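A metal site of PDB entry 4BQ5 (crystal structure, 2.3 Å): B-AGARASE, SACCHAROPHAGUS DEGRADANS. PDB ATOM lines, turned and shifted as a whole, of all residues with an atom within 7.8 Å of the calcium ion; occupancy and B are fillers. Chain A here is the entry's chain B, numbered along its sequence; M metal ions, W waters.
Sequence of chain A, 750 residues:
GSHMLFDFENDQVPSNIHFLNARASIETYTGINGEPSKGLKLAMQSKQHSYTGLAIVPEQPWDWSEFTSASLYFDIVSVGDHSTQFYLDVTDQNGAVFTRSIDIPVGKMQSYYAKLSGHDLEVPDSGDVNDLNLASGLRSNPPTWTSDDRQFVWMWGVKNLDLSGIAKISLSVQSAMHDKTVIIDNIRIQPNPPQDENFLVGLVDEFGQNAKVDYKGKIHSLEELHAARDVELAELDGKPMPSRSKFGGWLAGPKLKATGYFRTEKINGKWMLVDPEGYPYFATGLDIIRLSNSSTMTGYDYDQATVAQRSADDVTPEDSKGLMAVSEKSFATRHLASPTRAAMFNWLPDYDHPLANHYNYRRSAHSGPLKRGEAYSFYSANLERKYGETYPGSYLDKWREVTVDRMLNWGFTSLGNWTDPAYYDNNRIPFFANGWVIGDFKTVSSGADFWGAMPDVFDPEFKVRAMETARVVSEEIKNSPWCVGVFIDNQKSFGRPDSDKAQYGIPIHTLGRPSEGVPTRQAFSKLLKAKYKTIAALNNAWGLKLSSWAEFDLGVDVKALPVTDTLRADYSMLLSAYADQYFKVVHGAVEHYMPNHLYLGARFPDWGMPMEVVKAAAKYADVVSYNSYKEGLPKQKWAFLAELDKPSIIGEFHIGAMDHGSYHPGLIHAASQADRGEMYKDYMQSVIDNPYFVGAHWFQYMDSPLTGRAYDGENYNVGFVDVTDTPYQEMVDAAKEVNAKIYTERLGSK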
ATOM      1  N   HIS A 353     -10.501  -1.043   7.695  1.00  0.00           N
ATOM      2  CA  HIS A 353     -11.175  -2.071   8.478  1.00  0.00           C
ATOM      3  C   HIS A 353     -10.147  -3.084   9.056  1.00  0.00           C
ATOM      4  O   HIS A 353      -9.178  -3.417   8.387  1.00  0.00           O
ATOM      5  CB  HIS A 353     -12.263  -2.724   7.613  1.00  0.00           C
ATOM      6  CG  HIS A 353     -13.206  -3.596   8.384  1.00  0.00           C
ATOM      7  ND1 HIS A 353     -12.875  -4.864   8.833  1.00  0.00           N
ATOM      8  CD2 HIS A 353     -14.484  -3.386   8.796  1.00  0.00           C
ATOM      9  CE1 HIS A 353     -13.883  -5.384   9.488  1.00  0.00           C
ATOM     10  NE2 HIS A 353     -14.879  -4.516   9.474  1.00  0.00           N
ATOM     11  N   PRO A 354     -10.337  -3.528  10.305  1.00  0.00           N
ATOM     12  CA  PRO A 354      -9.470  -4.548  10.917  1.00  0.00           C
ATOM     13  C   PRO A 354      -9.196  -5.773   9.997  1.00  0.00           C
ATOM     14  O   PRO A 354      -8.071  -6.307   9.993  1.00  0.00           O
ATOM     15  CB  PRO A 354     -10.281  -5.050  12.128  1.00  0.00           C
ATOM     16  CG  PRO A 354     -11.292  -4.000  12.405  1.00  0.00           C
ATOM     17  CD  PRO A 354     -11.497  -3.191  11.155  1.00  0.00           C
ATOM     18  N   LEU A 355     -10.193  -6.198   9.227  1.00  0.00           N
ATOM     19  CA  LEU A 355     -10.060  -7.361   8.367  1.00  0.00           C
ATOM     20  C   LEU A 355      -9.580  -7.012   6.956  1.00  0.00           C
ATOM     21  O   LEU A 355      -9.628  -7.849   6.048  1.00  0.00           O
ATOM     22  CB  LEU A 355     -11.347  -8.196   8.355  1.00  0.00           C
ATOM     23  CG  LEU A 355     -11.930  -8.650   9.716  1.00  0.00           C
ATOM     24  CD1 LEU A 355     -13.270  -9.401   9.576  1.00  0.00           C
ATOM     25  CD2 LEU A 355     -10.919  -9.477  10.490  1.00  0.00           C
ATOM     26  N   ALA A 356      -9.084  -5.784   6.789  1.00  0.00           N
ATOM     27  CA  ALA A 356      -8.466  -5.313   5.541  1.00  0.00           C
ATOM     28  C   ALA A 356      -7.215  -6.083   5.110  1.00  0.00           C
ATOM     29  O   ALA A 356      -6.855  -6.068   3.937  1.00  0.00           O
ATOM     30  CB  ALA A 356      -8.125  -3.830   5.672  1.00  0.00           C
ATOM     31  N   ASN A 357      -6.545  -6.728   6.079  1.00  0.00           N
ATOM     32  CA  ASN A 357      -5.257  -7.354   5.845  1.00  0.00           C
ATOM     33  C   ASN A 357      -5.384  -8.764   5.283  1.00  0.00           C
ATOM     34  O   ASN A 357      -4.389  -9.467   5.092  1.00  0.00           O
ATOM     35  CB  ASN A 357      -4.403  -7.335   7.113  1.00  0.00           C
ATOM     36  CG  ASN A 357      -5.016  -8.107   8.247  1.00  0.00           C
ATOM     37  OD1 ASN A 357      -4.542  -9.185   8.618  1.00  0.00           O
ATOM     38  ND2 ASN A 357      -6.079  -7.567   8.822  1.00  0.00           N
ATOM     39  N   HIS A 358      -6.624  -9.145   4.975  1.00  0.00           N
ATOM     40  CA  HIS A 358      -6.900 -10.420   4.369  1.00  0.00           C
ATOM     41  C   HIS A 358      -7.082 -10.340   2.831  1.00  0.00           C
ATOM     42  O   HIS A 358      -7.318 -11.352   2.176  1.00  0.00           O
ATOM     43  CB  HIS A 358      -8.064 -11.073   5.098  1.00  0.00           C
ATOM     44  CG  HIS A 358      -7.805 -11.214   6.562  1.00  0.00           C
ATOM     45  ND1 HIS A 358      -6.941 -12.153   7.076  1.00  0.00           N
ATOM     46  CD2 HIS A 358      -8.214 -10.462   7.609  1.00  0.00           C
ATOM     47  CE1 HIS A 358      -6.859 -12.005   8.386  1.00  0.00           C
ATOM     48  NE2 HIS A 358      -7.625 -10.991   8.735  1.00  0.00           N
ATOM     49  N   GLU A 384      -8.857 -14.655  12.004  1.00  0.00           N
ATOM     50  CA  GLU A 384      -8.755 -13.450  12.809  1.00  0.00           C
ATOM     51  C   GLU A 384      -9.984 -13.260  13.685  1.00  0.00           C
ATOM     52  O   GLU A 384      -9.840 -12.932  14.860  1.00  0.00           O
ATOM     53  CB  GLU A 384      -8.507 -12.161  11.999  1.00  0.00           C
ATOM     54  CG  GLU A 384      -8.418 -10.935  12.941  1.00  0.00           C
ATOM     55  CD  GLU A 384      -7.879  -9.685  12.310  1.00  0.00           C
ATOM     56  OE1 GLU A 384      -7.375  -9.762  11.169  1.00  0.00           O
ATOM     57  OE2 GLU A 384      -7.957  -8.612  12.968  1.00  0.00           O
ATOM     58  N   GLY A 388      -8.567 -13.458  17.027  1.00  0.00           N
ATOM     59  CA  GLY A 388      -8.209 -12.075  17.306  1.00  0.00           C
ATOM     60  C   GLY A 388      -6.772 -11.744  16.942  1.00  0.00           C
ATOM     61  O   GLY A 388      -6.084 -12.535  16.276  1.00  0.00           O
ATOM     62  N   GLU A 389      -6.333 -10.569  17.383  1.00  0.00           N
ATOM     63  CA  GLU A 389      -4.903 -10.178  17.327  1.00  0.00           C
ATOM     64  C   GLU A 389      -4.462  -9.648  18.691  1.00  0.00           C
ATOM     65  O   GLU A 389      -5.070  -8.742  19.229  1.00  0.00           O
ATOM     66  CB  GLU A 389      -4.671  -9.138  16.245  1.00  0.00           C
ATOM     67  CG  GLU A 389      -4.487  -9.725  14.853  1.00  0.00           C
ATOM     68  CD  GLU A 389      -4.114  -8.678  13.814  1.00  0.00           C
ATOM     69  OE1 GLU A 389      -3.963  -7.516  14.231  1.00  0.00           O
ATOM     70  OE2 GLU A 389      -4.010  -8.993  12.589  1.00  0.00           O
ATOM     71  N   TYR A 391      -1.057  -9.504  18.777  1.00  0.00           N
ATOM     72  CA  TYR A 391       0.071  -8.933  18.073  1.00  0.00           C
ATOM     73  C   TYR A 391      -0.237  -9.213  16.604  1.00  0.00           C
ATOM     74  O   TYR A 391      -1.085 -10.039  16.308  1.00  0.00           O
ATOM     75  CB  TYR A 391       1.415  -9.538  18.527  1.00  0.00           C
ATOM     76  CG  TYR A 391       1.532 -11.059  18.413  1.00  0.00           C
ATOM     77  CD1 TYR A 391       1.913 -11.681  17.213  1.00  0.00           C
ATOM     78  CD2 TYR A 391       1.270 -11.875  19.525  1.00  0.00           C
ATOM     79  CE1 TYR A 391       2.014 -13.069  17.117  1.00  0.00           C
ATOM     80  CE2 TYR A 391       1.376 -13.256  19.433  1.00  0.00           C
ATOM     81  CZ  TYR A 391       1.751 -13.843  18.233  1.00  0.00           C
ATOM     82  OH  TYR A 391       1.860 -15.198  18.161  1.00  0.00           O
ATOM     83  N   PRO A 392       0.445  -8.511  15.679  1.00  0.00           N
ATOM     84  CA  PRO A 392       0.149  -8.745  14.253  1.00  0.00           C
ATOM     85  C   PRO A 392       0.326 -10.207  13.801  1.00  0.00           C
ATOM     86  O   PRO A 392       1.402 -10.789  13.960  1.00  0.00           O
ATOM     87  CB  PRO A 392       1.104  -7.777  13.519  1.00  0.00           C
ATOM     88  CG  PRO A 392       1.562  -6.813  14.545  1.00  0.00           C
ATOM     89  CD  PRO A 392       1.496  -7.497  15.882  1.00  0.00           C
ATOM     90  N   GLY A 393      -0.734 -10.777  13.237  1.00  0.00           N
ATOM     91  CA  GLY A 393      -0.729 -12.182  12.804  1.00  0.00           C
ATOM     92  C   GLY A 393      -0.788 -13.232  13.900  1.00  0.00           C
ATOM     93  O   GLY A 393      -0.597 -14.434  13.614  1.00  0.00           O
ATOM     94  N   TYR A 395      -3.161 -14.585  15.180  1.00  0.00           N
ATOM     95  CA  TYR A 395      -4.171 -15.577  14.855  1.00  0.00           C
ATOM     96  C   TYR A 395      -3.572 -16.608  13.882  1.00  0.00           C
ATOM     97  O   TYR A 395      -4.081 -17.718  13.801  1.00  0.00           O
ATOM     98  CB  TYR A 395      -5.398 -14.895  14.247  1.00  0.00           C
ATOM     99  CG  TYR A 395      -5.064 -14.046  13.043  1.00  0.00           C
ATOM    100  CD1 TYR A 395      -5.012 -14.589  11.743  1.00  0.00           C
ATOM    101  CD2 TYR A 395      -4.769 -12.694  13.196  1.00  0.00           C
ATOM    102  CE1 TYR A 395      -4.667 -13.806  10.631  1.00  0.00           C
ATOM    103  CE2 TYR A 395      -4.433 -11.907  12.105  1.00  0.00           C
ATOM    104  CZ  TYR A 395      -4.399 -12.459  10.815  1.00  0.00           C
ATOM    105  OH  TYR A 395      -4.076 -11.645   9.742  1.00  0.00           O
HETATM  106 CA    CA M   1      -6.256  -7.467  11.176  1.00  0.00          CA
HETATM  107  O   HOH W   1      -5.322  -5.204  10.502  1.00  0.00           O
HETATM  108  O   HOH W   2      -6.371  -5.896  13.101  1.00  0.00           O
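The side-chain amide oxygen of Asn 357 is in hydrogen-bond range of the side-chain hydroxyl of Tyr 395 (2.7 Å).
OE1 of Glu 384 lies close to NE2 of His 358 (2.7 Å).
Within 4 Å of the calcium ion: Pro 354, Asn 357, Glu 384 and Glu 389.
The nearest printed residue that does not touch the calcium ion is His 358 (4.5 Å).
The calcium ion is bound by the side-chain amide nitrogen (ND2) of Asn 357, at 2.4 Å.
The backbone carbonyl oxygen (O) of Pro 354 binds the calcium ion (2.5 Å).
The calcium ion is bound by water W2 (2.5 Å).
Water W1 binds the calcium ion (2.5 Å).
The calcium ion is bound by the side-chain carboxylate (OE1) of Glu 384 (2.6 Å).
The calcium ion is bound by the side-chain carboxylate (OE2) of Glu 384, 2.7 Å away.
The calcium ion has six donor atoms within binding distance.
Slightly farther from the calcium ion lies OE2 of Glu 389 (3.1 Å).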
